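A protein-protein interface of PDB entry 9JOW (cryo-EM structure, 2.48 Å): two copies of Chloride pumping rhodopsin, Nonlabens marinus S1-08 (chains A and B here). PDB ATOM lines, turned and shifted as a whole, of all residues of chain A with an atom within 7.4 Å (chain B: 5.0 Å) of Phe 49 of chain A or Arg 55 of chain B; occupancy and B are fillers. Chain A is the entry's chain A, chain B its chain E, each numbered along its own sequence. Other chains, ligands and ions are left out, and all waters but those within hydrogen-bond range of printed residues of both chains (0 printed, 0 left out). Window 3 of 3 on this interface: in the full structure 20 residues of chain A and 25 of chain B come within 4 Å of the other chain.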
ATOM      1  N   PHE A  42     -22.198 -20.254  31.658  1.00  0.00           N
ATOM      2  CA  PHE A  42     -21.525 -20.770  30.482  1.00  0.00           C
ATOM      3  C   PHE A  42     -21.991 -20.067  29.217  1.00  0.00           C
ATOM      4  O   PHE A  42     -21.151 -19.635  28.431  1.00  0.00           O
ATOM      5  CB  PHE A  42     -21.772 -22.266  30.365  1.00  0.00           C
ATOM      6  CG  PHE A  42     -21.082 -22.892  29.174  1.00  0.00           C
ATOM      7  CD1 PHE A  42     -21.727 -22.977  27.956  1.00  0.00           C
ATOM      8  CD2 PHE A  42     -19.790 -23.406  29.288  1.00  0.00           C
ATOM      9  CE1 PHE A  42     -21.122 -23.604  26.868  1.00  0.00           C
ATOM     10  CE2 PHE A  42     -19.149 -23.950  28.179  1.00  0.00           C
ATOM     11  CZ  PHE A  42     -19.847 -24.096  26.980  1.00  0.00           C
ATOM     12  N   LEU A  44     -23.210 -17.099  28.905  1.00  0.00           N
ATOM     13  CA  LEU A  44     -22.701 -15.731  28.816  1.00  0.00           C
ATOM     14  C   LEU A  44     -21.244 -15.715  28.370  1.00  0.00           C
ATOM     15  O   LEU A  44     -20.906 -15.014  27.422  1.00  0.00           O
ATOM     16  CB  LEU A  44     -22.933 -14.994  30.133  1.00  0.00           C
ATOM     17  CG  LEU A  44     -24.425 -14.818  30.462  1.00  0.00           C
ATOM     18  CD1 LEU A  44     -24.578 -14.432  31.852  1.00  0.00           C
ATOM     19  CD2 LEU A  44     -25.171 -13.830  29.612  1.00  0.00           C
ATOM     20  N   VAL A  45     -20.390 -16.528  28.986  1.00  0.00           N
ATOM     21  CA  VAL A  45     -18.986 -16.566  28.581  1.00  0.00           C
ATOM     22  C   VAL A  45     -18.769 -16.951  27.102  1.00  0.00           C
ATOM     23  O   VAL A  45     -17.889 -16.389  26.479  1.00  0.00           O
ATOM     24  CB  VAL A  45     -18.188 -17.537  29.445  1.00  0.00           C
ATOM     25  CG1 VAL A  45     -16.786 -17.708  28.925  1.00  0.00           C
ATOM     26  CG2 VAL A  45     -18.163 -17.094  30.872  1.00  0.00           C
ATOM     27  N   VAL A  46     -19.476 -17.919  26.537  1.00  0.00           N
ATOM     28  CA  VAL A  46     -19.171 -18.327  25.175  1.00  0.00           C
ATOM     29  C   VAL A  46     -19.948 -17.501  24.155  1.00  0.00           C
ATOM     30  O   VAL A  46     -19.679 -17.623  22.970  1.00  0.00           O
ATOM     31  CB  VAL A  46     -19.411 -19.832  24.887  1.00  0.00           C
ATOM     32  CG1 VAL A  46     -18.705 -20.679  25.929  1.00  0.00           C
ATOM     33  CG2 VAL A  46     -20.888 -20.163  24.846  1.00  0.00           C
ATOM     34  N   SER A  47     -20.903 -16.672  24.580  1.00  0.00           N
ATOM     35  CA  SER A  47     -21.601 -15.821  23.618  1.00  0.00           C
ATOM     36  C   SER A  47     -20.648 -14.943  22.790  1.00  0.00           C
ATOM     37  O   SER A  47     -20.961 -14.583  21.663  1.00  0.00           O
ATOM     38  CB  SER A  47     -22.573 -14.932  24.308  1.00  0.00           C
ATOM     39  OG  SER A  47     -21.917 -14.068  25.233  1.00  0.00           O
ATOM     40  N   GLN A  48     -19.459 -14.609  23.308  1.00  0.00           N
ATOM     41  CA  GLN A  48     -18.556 -13.775  22.534  1.00  0.00           C
ATOM     42  C   GLN A  48     -18.006 -14.462  21.274  1.00  0.00           C
ATOM     43  O   GLN A  48     -17.576 -13.795  20.349  1.00  0.00           O
ATOM     44  CB  GLN A  48     -17.429 -13.235  23.392  1.00  0.00           C
ATOM     45  CG  GLN A  48     -16.326 -14.223  23.715  1.00  0.00           C
ATOM     46  CD  GLN A  48     -15.498 -13.714  24.880  1.00  0.00           C
ATOM     47  OE1 GLN A  48     -14.924 -12.618  24.782  1.00  0.00           O
ATOM     48  NE2 GLN A  48     -15.453 -14.455  25.994  1.00  0.00           N
ATOM     49  N   PHE A  49     -18.066 -15.781  21.217  1.00  0.00           N
ATOM     50  CA  PHE A  49     -17.634 -16.492  20.043  1.00  0.00           C
ATOM     51  C   PHE A  49     -18.755 -16.705  19.042  1.00  0.00           C
ATOM     52  O   PHE A  49     -18.523 -17.378  18.031  1.00  0.00           O
ATOM     53  CB  PHE A  49     -17.146 -17.895  20.380  1.00  0.00           C
ATOM     54  CG  PHE A  49     -16.115 -17.856  21.481  1.00  0.00           C
ATOM     55  CD1 PHE A  49     -15.179 -16.837  21.511  1.00  0.00           C
ATOM     56  CD2 PHE A  49     -16.076 -18.846  22.454  1.00  0.00           C
ATOM     57  CE1 PHE A  49     -14.243 -16.769  22.544  1.00  0.00           C
ATOM     58  CE2 PHE A  49     -15.144 -18.784  23.461  1.00  0.00           C
ATOM     59  CZ  PHE A  49     -14.233 -17.739  23.511  1.00  0.00           C
ATOM     60  N   VAL A  50     -19.946 -16.152  19.255  1.00  0.00           N
ATOM     61  CA  VAL A  50     -20.987 -16.347  18.251  1.00  0.00           C
ATOM     62  C   VAL A  50     -21.054 -15.079  17.436  1.00  0.00           C
ATOM     63  O   VAL A  50     -21.001 -14.008  18.026  1.00  0.00           O
ATOM     64  CB  VAL A  50     -22.294 -16.630  19.006  1.00  0.00           C
ATOM     65  CG1 VAL A  50     -23.474 -16.778  18.068  1.00  0.00           C
ATOM     66  CG2 VAL A  50     -22.176 -17.877  19.857  1.00  0.00           C
ATOM     67  N   ALA A  51     -21.212 -15.157  16.121  1.00  0.00           N
ATOM     68  CA  ALA A  51     -21.400 -13.914  15.360  1.00  0.00           C
ATOM     69  C   ALA A  51     -22.723 -13.226  15.717  1.00  0.00           C
ATOM     70  O   ALA A  51     -23.714 -13.891  15.971  1.00  0.00           O
ATOM     71  CB  ALA A  51     -21.381 -14.245  13.923  1.00  0.00           C
ATOM     72  N   PRO A  52     -22.790 -11.893  15.730  1.00  0.00           N
ATOM     73  CA  PRO A  52     -24.003 -11.140  16.064  1.00  0.00           C
ATOM     74  C   PRO A  52     -25.306 -11.584  15.404  1.00  0.00           C
ATOM     75  O   PRO A  52     -26.369 -11.586  16.042  1.00  0.00           O
ATOM     76  CB  PRO A  52     -23.745  -9.744  15.491  1.00  0.00           C
ATOM     77  CG  PRO A  52     -22.247  -9.652  15.684  1.00  0.00           C
ATOM     78  CD  PRO A  52     -21.642 -11.022  15.473  1.00  0.00           C
ATOM     79  N   ARG A  55     -26.264 -14.313  17.678  1.00  0.00           N
ATOM     80  CA  ARG A  55     -26.098 -14.178  19.116  1.00  0.00           C
ATOM     81  C   ARG A  55     -27.451 -14.092  19.849  1.00  0.00           C
ATOM     82  O   ARG A  55     -27.553 -14.398  21.024  1.00  0.00           O
ATOM     83  CB  ARG A  55     -25.190 -12.975  19.421  1.00  0.00           C
ATOM     84  CG  ARG A  55     -24.666 -13.100  20.846  1.00  0.00           C
ATOM     85  CD  ARG A  55     -23.559 -12.161  21.203  1.00  0.00           C
ATOM     86  NE  ARG A  55     -22.513 -12.252  20.189  1.00  0.00           N
ATOM     87  CZ  ARG A  55     -21.715 -11.285  19.892  1.00  0.00           C
ATOM     88  NH1 ARG A  55     -21.863 -10.130  20.472  1.00  0.00           N
ATOM     89  NH2 ARG A  55     -20.794 -11.466  18.974  1.00  0.00           N
ATOM     90  N   THR A 250     -25.975 -23.729  20.624  1.00  0.00           N
ATOM     91  CA  THR A 250     -24.851 -22.825  20.680  1.00  0.00           C
ATOM     92  C   THR A 250     -23.697 -23.393  19.867  1.00  0.00           C
ATOM     93  O   THR A 250     -23.020 -22.668  19.152  1.00  0.00           O
ATOM     94  CB  THR A 250     -24.431 -22.514  22.126  1.00  0.00           C
ATOM     95  OG1 THR A 250     -25.248 -21.439  22.564  1.00  0.00           O
ATOM     96  CG2 THR A 250     -23.125 -21.759  22.197  1.00  0.00           C
ATOM     97  N   ALA A 253     -24.482 -22.661  16.308  1.00  0.00           N
ATOM     98  CA  ALA A 253     -24.214 -21.238  16.064  1.00  0.00           C
ATOM     99  C   ALA A 253     -22.713 -20.911  15.909  1.00  0.00           C
ATOM    100  O   ALA A 253     -22.317 -20.091  15.072  1.00  0.00           O
ATOM    101  CB  ALA A 253     -24.807 -20.422  17.182  1.00  0.00           C
ATOM    102  N   ILE A 254     -21.858 -21.542  16.715  1.00  0.00           N
ATOM    103  CA  ILE A 254     -20.436 -21.287  16.609  1.00  0.00           C
ATOM    104  C   ILE A 254     -19.876 -21.841  15.296  1.00  0.00           C
ATOM    105  O   ILE A 254     -19.140 -21.145  14.597  1.00  0.00           O
ATOM    106  CB  ILE A 254     -19.676 -21.736  17.867  1.00  0.00           C
ATOM    107  CG1 ILE A 254     -20.118 -20.917  19.041  1.00  0.00           C
ATOM    108  CG2 ILE A 254     -18.183 -21.503  17.691  1.00  0.00           C
ATOM    109  CD1 ILE A 254     -19.595 -21.356  20.390  1.00  0.00           C
ATOM    110  N   GLN A 255     -20.235 -23.064  14.953  1.00  0.00           N
ATOM    111  CA  GLN A 255     -19.785 -23.667  13.706  1.00  0.00           C
ATOM    112  C   GLN A 255     -20.201 -22.854  12.486  1.00  0.00           C
ATOM    113  O   GLN A 255     -19.390 -22.641  11.578  1.00  0.00           O
ATOM    114  CB  GLN A 255     -20.388 -25.036  13.467  1.00  0.00           C
ATOM    115  CG  GLN A 255     -19.878 -26.106  14.421  1.00  0.00           C
ATOM    116  CD  GLN A 255     -18.410 -26.371  14.240  1.00  0.00           C
ATOM    117  OE1 GLN A 255     -17.881 -26.307  13.125  1.00  0.00           O
ATOM    118  NE2 GLN A 255     -17.759 -26.716  15.339  1.00  0.00           N
ATOM    119  N   SER A 257     -20.993 -19.623  12.522  1.00  0.00           N
ATOM    120  CA  SER A 257     -20.315 -18.348  12.578  1.00  0.00           C
ATOM    121  C   SER A 257     -18.932 -18.466  11.943  1.00  0.00           C
ATOM    122  O   SER A 257     -18.444 -17.559  11.282  1.00  0.00           O
ATOM    123  CB  SER A 257     -20.193 -17.834  14.012  1.00  0.00           C
ATOM    124  OG  SER A 257     -21.458 -17.571  14.605  1.00  0.00           O
ATOM    125  N   ALA A 258     -18.248 -19.546  12.250  1.00  0.00           N
ATOM    126  CA  ALA A 258     -16.883 -19.678  11.796  1.00  0.00           C
ATOM    127  C   ALA A 258     -16.903 -19.845  10.289  1.00  0.00           C
ATOM    128  O   ALA A 258     -16.115 -19.212   9.590  1.00  0.00           O
ATOM    129  CB  ALA A 258     -16.207 -20.826  12.463  1.00  0.00           C
ATOM    130  N   TYR A 262     -16.528 -15.296  10.906  1.00  0.00           N
ATOM    131  CA  TYR A 262     -16.355 -14.554  12.141  1.00  0.00           C
ATOM    132  C   TYR A 262     -15.112 -15.069  12.847  1.00  0.00           C
ATOM    133  O   TYR A 262     -14.934 -16.260  13.068  1.00  0.00           O
ATOM    134  CB  TYR A 262     -17.639 -14.730  12.921  1.00  0.00           C
ATOM    135  CG  TYR A 262     -17.678 -13.953  14.208  1.00  0.00           C
ATOM    136  CD1 TYR A 262     -17.806 -12.593  14.185  1.00  0.00           C
ATOM    137  CD2 TYR A 262     -17.710 -14.600  15.437  1.00  0.00           C
ATOM    138  CE1 TYR A 262     -17.911 -11.866  15.356  1.00  0.00           C
ATOM    139  CE2 TYR A 262     -17.800 -13.883  16.621  1.00  0.00           C
ATOM    140  CZ  TYR A 262     -17.894 -12.503  16.578  1.00  0.00           C
ATOM    141  OH  TYR A 262     -17.961 -11.743  17.703  1.00  0.00           O
ATOM    142  N   VAL A 263     -14.205 -14.166  13.154  1.00  0.00           N
ATOM    143  CA  VAL A 263     -12.888 -14.602  13.539  1.00  0.00           C
ATOM    144  C   VAL A 263     -12.885 -15.179  14.943  1.00  0.00           C
ATOM    145  O   VAL A 263     -12.384 -16.290  15.141  1.00  0.00           O
ATOM    146  CB  VAL A 263     -11.874 -13.470  13.368  1.00  0.00           C
ATOM    147  CG1 VAL A 263     -10.605 -13.841  14.087  1.00  0.00           C
ATOM    148  CG2 VAL A 263     -11.624 -13.241  11.889  1.00  0.00           C
ATOM    149  N   PRO A 264     -13.490 -14.503  15.935  1.00  0.00           N
ATOM    150  CA  PRO A 264     -13.617 -15.095  17.270  1.00  0.00           C
ATOM    151  C   PRO A 264     -14.119 -16.540  17.249  1.00  0.00           C
ATOM    152  O   PRO A 264     -13.618 -17.396  17.970  1.00  0.00           O
ATOM    153  CB  PRO A 264     -14.611 -14.212  17.977  1.00  0.00           C
ATOM    154  CG  PRO A 264     -14.539 -12.894  17.208  1.00  0.00           C
ATOM    155  CD  PRO A 264     -14.210 -13.232  15.795  1.00  0.00           C
ATOM    156  N   ALA A 265     -15.053 -16.841  16.351  1.00  0.00           N
ATOM    157  CA  ALA A 265     -15.512 -18.210  16.219  1.00  0.00           C
ATOM    158  C   ALA A 265     -14.415 -19.069  15.628  1.00  0.00           C
ATOM    159  O   ALA A 265     -14.311 -20.221  16.010  1.00  0.00           O
ATOM    160  CB  ALA A 265     -16.791 -18.292  15.396  1.00  0.00           C
ATOM    161  N   GLN A 266     -13.683 -18.560  14.631  1.00  0.00           N
ATOM    162  CA  GLN A 266     -12.639 -19.377  14.025  1.00  0.00           C
ATOM    163  C   GLN A 266     -11.561 -19.670  15.062  1.00  0.00           C
ATOM    164  O   GLN A 266     -11.189 -20.822  15.245  1.00  0.00           O
ATOM    165  CB  GLN A 266     -12.051 -18.663  12.819  1.00  0.00           C
ATOM    166  CG  GLN A 266     -12.895 -18.849  11.579  1.00  0.00           C
ATOM    167  CD  GLN A 266     -12.632 -17.823  10.514  1.00  0.00           C
ATOM    168  OE1 GLN A 266     -11.881 -16.860  10.697  1.00  0.00           O
ATOM    169  NE2 GLN A 266     -13.290 -18.030   9.386  1.00  0.00           N
ATOM    170  N   GLN A 267     -11.145 -18.644  15.815  1.00  0.00           N
ATOM    171  CA  GLN A 267     -10.256 -18.825  16.959  1.00  0.00           C
ATOM    172  C   GLN A 267     -10.815 -19.846  17.953  1.00  0.00           C
ATOM    173  O   GLN A 267     -10.128 -20.764  18.357  1.00  0.00           O
ATOM    174  CB  GLN A 267     -10.049 -17.490  17.665  1.00  0.00           C
ATOM    175  CG  GLN A 267      -9.228 -16.503  16.836  1.00  0.00           C
ATOM    176  CD  GLN A 267      -9.074 -15.149  17.473  1.00  0.00           C
ATOM    177  OE1 GLN A 267      -9.858 -14.732  18.335  1.00  0.00           O
ATOM    178  NE2 GLN A 267      -8.094 -14.410  16.974  1.00  0.00           N
ATOM    179  N   ALA A 268     -12.091 -19.742  18.319  1.00  0.00           N
ATOM    180  CA  ALA A 268     -12.623 -20.666  19.307  1.00  0.00           C
ATOM    181  C   ALA A 268     -12.499 -22.102  18.822  1.00  0.00           C
ATOM    182  O   ALA A 268     -12.461 -23.015  19.624  1.00  0.00           O
ATOM    183  CB  ALA A 268     -14.052 -20.341  19.671  1.00  0.00           C
ATOM    184  N   LEU A 269     -12.483 -22.316  17.519  1.00  0.00           N
ATOM    185  CA  LEU A 269     -12.372 -23.663  16.987  1.00  0.00           C
ATOM    186  C   LEU A 269     -10.932 -24.003  16.615  1.00  0.00           C
ATOM    187  O   LEU A 269     -10.705 -25.069  16.067  1.00  0.00           O
ATOM    188  CB  LEU A 269     -13.255 -23.787  15.748  1.00  0.00           C
ATOM    189  CG  LEU A 269     -14.757 -23.672  15.969  1.00  0.00           C
ATOM    190  CD1 LEU A 269     -15.497 -23.720  14.673  1.00  0.00           C
ATOM    191  CD2 LEU A 269     -15.253 -24.788  16.835  1.00  0.00           C
ATOM    192  N   SER B  47     -10.486 -15.090  32.807  1.00  0.00           N
ATOM    193  CA  SER B  47     -10.789 -15.702  31.526  1.00  0.00           C
ATOM    194  C   SER B  47     -10.282 -14.888  30.336  1.00  0.00           C
ATOM    195  O   SER B  47      -9.996 -15.444  29.283  1.00  0.00           O
ATOM    196  CB  SER B  47     -12.252 -15.947  31.379  1.00  0.00           C
ATOM    197  OG  SER B  47     -12.959 -14.727  31.442  1.00  0.00           O
ATOM    198  N   GLN B  48     -10.174 -13.568  30.478  1.00  0.00           N
ATOM    199  CA  GLN B  48      -9.754 -12.748  29.350  1.00  0.00           C
ATOM    200  C   GLN B  48      -8.301 -12.985  28.949  1.00  0.00           C
ATOM    201  O   GLN B  48      -7.934 -12.694  27.821  1.00  0.00           O
ATOM    202  CB  GLN B  48     -10.005 -11.273  29.601  1.00  0.00           C
ATOM    203  CG  GLN B  48      -9.025 -10.592  30.540  1.00  0.00           C
ATOM    204  CD  GLN B  48      -9.592  -9.283  31.028  1.00  0.00           C
ATOM    205  OE1 GLN B  48      -9.979  -8.433  30.211  1.00  0.00           O
ATOM    206  NE2 GLN B  48      -9.689  -9.134  32.346  1.00  0.00           N
ATOM    207  N   VAL B  50      -7.070 -16.018  28.629  1.00  0.00           N
ATOM    208  CA  VAL B  50      -6.902 -17.347  28.058  1.00  0.00           C
ATOM    209  C   VAL B  50      -7.257 -17.219  26.590  1.00  0.00           C
ATOM    210  O   VAL B  50      -8.221 -16.535  26.276  1.00  0.00           O
ATOM    211  CB  VAL B  50      -7.849 -18.311  28.785  1.00  0.00           C
ATOM    212  CG1 VAL B  50      -7.856 -19.693  28.170  1.00  0.00           C
ATOM    213  CG2 VAL B  50      -7.537 -18.387  30.251  1.00  0.00           C
ATOM    214  N   ALA B  51      -6.519 -17.850  25.689  1.00  0.00           N
ATOM    215  CA  ALA B  51      -6.912 -17.785  24.281  1.00  0.00           C
ATOM    216  C   ALA B  51      -8.234 -18.512  24.057  1.00  0.00           C
ATOM    217  O   ALA B  51      -8.472 -19.543  24.655  1.00  0.00           O
ATOM    218  CB  ALA B  51      -5.854 -18.403  23.453  1.00  0.00           C
ATOM    219  N   PRO B  52      -9.103 -18.035  23.146  1.00  0.00           N
ATOM    220  CA  PRO B  52     -10.367 -18.676  22.815  1.00  0.00           C
ATOM    221  C   PRO B  52     -10.352 -20.188  22.604  1.00  0.00           C
ATOM    222  O   PRO B  52     -11.305 -20.852  23.041  1.00  0.00           O
ATOM    223  CB  PRO B  52     -10.749 -18.067  21.498  1.00  0.00           C
ATOM    224  CG  PRO B  52     -10.054 -16.749  21.508  1.00  0.00           C
ATOM    225  CD  PRO B  52      -8.872 -16.820  22.373  1.00  0.00           C
ATOM    226  N   LYS B  53      -9.283 -20.735  21.984  1.00  0.00           N
ATOM    227  CA  LYS B  53      -9.224 -22.187  21.803  1.00  0.00           C
ATOM    228  C   LYS B  53      -9.209 -22.942  23.148  1.00  0.00           C
ATOM    229  O   LYS B  53      -9.508 -24.119  23.178  1.00  0.00           O
ATOM    230  CB  LYS B  53      -8.078 -22.691  20.928  1.00  0.00           C
ATOM    231  CG  LYS B  53      -6.687 -22.551  21.446  1.00  0.00           C
ATOM    232  CD  LYS B  53      -5.783 -23.730  21.124  1.00  0.00           C
ATOM    233  CE  LYS B  53      -5.048 -23.589  19.867  1.00  0.00           C
ATOM    234  NZ  LYS B  53      -4.246 -24.792  19.634  1.00  0.00           N
ATOM    235  N   TYR B  54      -8.814 -22.291  24.253  1.00  0.00           N
ATOM    236  CA  TYR B  54      -8.833 -22.910  25.577  1.00  0.00           C
ATOM    237  C   TYR B  54      -9.862 -22.294  26.526  1.00  0.00           C
ATOM    238  O   TYR B  54     -10.015 -22.769  27.631  1.00  0.00           O
ATOM    239  CB  TYR B  54      -7.504 -22.730  26.298  1.00  0.00           C
ATOM    240  CG  TYR B  54      -6.344 -23.389  25.581  1.00  0.00           C
ATOM    241  CD1 TYR B  54      -6.276 -24.752  25.485  1.00  0.00           C
ATOM    242  CD2 TYR B  54      -5.300 -22.667  25.049  1.00  0.00           C
ATOM    243  CE1 TYR B  54      -5.190 -25.390  24.923  1.00  0.00           C
ATOM    244  CE2 TYR B  54      -4.219 -23.281  24.448  1.00  0.00           C
ATOM    245  CZ  TYR B  54      -4.166 -24.652  24.378  1.00  0.00           C
ATOM    246  OH  TYR B  54      -3.130 -25.312  23.798  1.00  0.00           O
ATOM    247  N   ARG B  55     -10.597 -21.268  26.101  1.00  0.00           N
ATOM    248  CA  ARG B  55     -11.452 -20.561  27.023  1.00  0.00           C
ATOM    249  C   ARG B  55     -12.631 -21.413  27.501  1.00  0.00           C
ATOM    250  O   ARG B  55     -13.190 -21.196  28.576  1.00  0.00           O
ATOM    251  CB  ARG B  55     -11.893 -19.218  26.447  1.00  0.00           C
ATOM    252  CG  ARG B  55     -12.346 -18.307  27.576  1.00  0.00           C
ATOM    253  CD  ARG B  55     -12.567 -16.898  27.209  1.00  0.00           C
ATOM    254  NE  ARG B  55     -11.356 -16.371  26.596  1.00  0.00           N
ATOM    255  CZ  ARG B  55     -11.353 -15.450  25.695  1.00  0.00           C
ATOM    256  NH1 ARG B  55     -12.494 -14.929  25.300  1.00  0.00           N
ATOM    257  NH2 ARG B  55     -10.217 -15.040  25.203  1.00  0.00           N
ATOM    258  N   ILE B  56     -12.992 -22.446  26.769  1.00  0.00           N
ATOM    259  CA  ILE B  56     -14.057 -23.345  27.217  1.00  0.00           C
ATOM    260  C   ILE B  56     -13.615 -23.957  28.544  1.00  0.00           C
ATOM    261  O   ILE B  56     -14.414 -24.104  29.446  1.00  0.00           O
ATOM    262  CB  ILE B  56     -14.362 -24.385  26.112  1.00  0.00           C
ATOM    263  CG1 ILE B  56     -14.447 -23.731  24.719  1.00  0.00           C
ATOM    264  CG2 ILE B  56     -15.625 -25.165  26.363  1.00  0.00           C
ATOM    265  CD1 ILE B  56     -13.157 -23.791  23.900  1.00  0.00           C
ATOM    266  N   ALA B  57     -12.325 -24.296  28.688  1.00  0.00           N
ATOM    267  CA  ALA B  57     -11.856 -24.935  29.901  1.00  0.00           C
ATOM    268  C   ALA B  57     -12.147 -24.017  31.079  1.00  0.00           C
ATOM    269  O   ALA B  57     -12.661 -24.475  32.092  1.00  0.00           O
ATOM    270  CB  ALA B  57     -10.381 -25.305  29.820  1.00  0.00           C
ATOM    271  N   THR B  58     -11.890 -22.725  30.940  1.00  0.00           N
ATOM    272  CA  THR B  58     -12.159 -21.833  32.054  1.00  0.00           C
ATOM    273  C   THR B  58     -13.672 -21.707  32.279  1.00  0.00           C
ATOM    274  O   THR B  58     -14.113 -21.662  33.413  1.00  0.00           O
ATOM    275  CB  THR B  58     -11.436 -20.498  31.824  1.00  0.00           C
ATOM    276  OG1 THR B  58     -10.077 -20.873  31.690  1.00  0.00           O
ATOM    277  CG2 THR B  58     -11.487 -19.560  33.014  1.00  0.00           C
ATOM    278  N   ALA B  59     -14.477 -21.671  31.217  1.00  0.00           N
ATOM    279  CA  ALA B  59     -15.923 -21.618  31.373  1.00  0.00           C
ATOM    280  C   ALA B  59     -16.462 -22.839  32.115  1.00  0.00           C
ATOM    281  O   ALA B  59     -17.391 -22.741  32.897  1.00  0.00           O
ATOM    282  CB  ALA B  59     -16.596 -21.529  30.011  1.00  0.00           C
ATOM    283  N   TYR B 262      -0.817 -15.735  22.125  1.00  0.00           N
ATOM    284  CA  TYR B 262      -1.945 -14.878  22.463  1.00  0.00           C
ATOM    285  C   TYR B 262      -1.426 -13.761  23.359  1.00  0.00           C
ATOM    286  O   TYR B 262      -0.740 -13.987  24.354  1.00  0.00           O
ATOM    287  CB  TYR B 262      -2.995 -15.776  23.079  1.00  0.00           C
ATOM    288  CG  TYR B 262      -4.246 -15.055  23.500  1.00  0.00           C
ATOM    289  CD1 TYR B 262      -5.122 -14.638  22.546  1.00  0.00           C
ATOM    290  CD2 TYR B 262      -4.603 -14.891  24.845  1.00  0.00           C
ATOM    291  CE1 TYR B 262      -6.324 -14.015  22.888  1.00  0.00           C
ATOM    292  CE2 TYR B 262      -5.789 -14.263  25.195  1.00  0.00           C
ATOM    293  CZ  TYR B 262      -6.653 -13.818  24.206  1.00  0.00           C
ATOM    294  OH  TYR B 262      -7.813 -13.180  24.481  1.00  0.00           O
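CD2 of Phe 42 of chain A touches CB of Ala 59 of chain B, at 3.8 Å.
CG1 of Val 45 of chain A touches CB of Ala 59 of chain B, 3.98 Å away.
Pro 52 of chain B touches Phe 49 of chain A (CB to CE1, 3.9 Å).
Arg 55 of chain B touches Phe 49 of chain A (NH1 to CE1, 3.7 Å).
Gln 267 of chain A touches Pro 52 of chain B.
Lys 53 of chain B touches Gln 267 of chain A.
Pro 52 of chain B touches Ala 268 of chain A.
Ala 268 of chain A touches Lys 53 of chain B.
NE2 of Gln 48 of chain A lies close to NH1 of Arg 55 of chain B (3.1 Å).
Printed residues of chain B that touch a printed residue of chain A: Pro 52, Lys 53, Arg 55 and Ala 59.
Among the printed residues, 9 pairs touch across the chains.
Among the printed residues, no Asp or Glu carboxylate lies within 4 Å of a Lys or Arg side-chain nitrogen of the other chain.
O of Val 45 of chain A is in hydrogen-bond range of NE2 of Gln 48 of chain A.
The backbone carbonyl oxygen (O) of Gln 48 of chain A is in hydrogen-bond range of the side-chain hydroxyl (OH) of Tyr 262 of chain A (3.4 Å).
The guanidinium group of Arg 55 of chain B sits at hydrogen-bond distance from the backbone carbonyl oxygen of Ser 47 of chain B, 3.2 Å away.
NH2 of Arg 55 of chain B sits at hydrogen-bond distance from O of Val 50 of chain B, 2.7 Å away.
The guanidinium group of Arg 55 of chain B sits at hydrogen-bond distance from the side-chain hydroxyl of Tyr 262 of chain B.
Of chain B, only Pro 52 and Arg 55 come within 4 Å of Phe 49 of chain A.
Arg 55 of chain B touches just these residues of chain A: Gln 48 and Phe 49.
Of the printed residues of chain A, Lys 53 of chain B touches Gln 267 and Ala 268.
Printed residues of chain B within 4 Å of Ala 268 of chain A: Pro 52 and Lys 53.
Of the printed residues of chain B, Val 45 of chain A touches Ala 59 (3.98 Å).
Printed residues of chain B within 4 Å of Gln 267 of chain A: Pro 52 and Lys 53.
Gln 255 of chain A touches none of the printed residues of chain B.
The nearest residue of chain A that does not touch Arg 55 of chain B is Val 45 of chain A (4.6 Å).
Gln 48 of chain A touches Arg 55 of chain B, but with the chains exchanged Arg 55 of chain A does not touch Gln 48 of chain B (15.0 Å).
Positions printed for both chains: 47, 48, 50, 51, 52, 55 and 262.
Of the 9 pairs that touch across the chains among the printed residues, none has its exchanged pair printed and touching as well.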
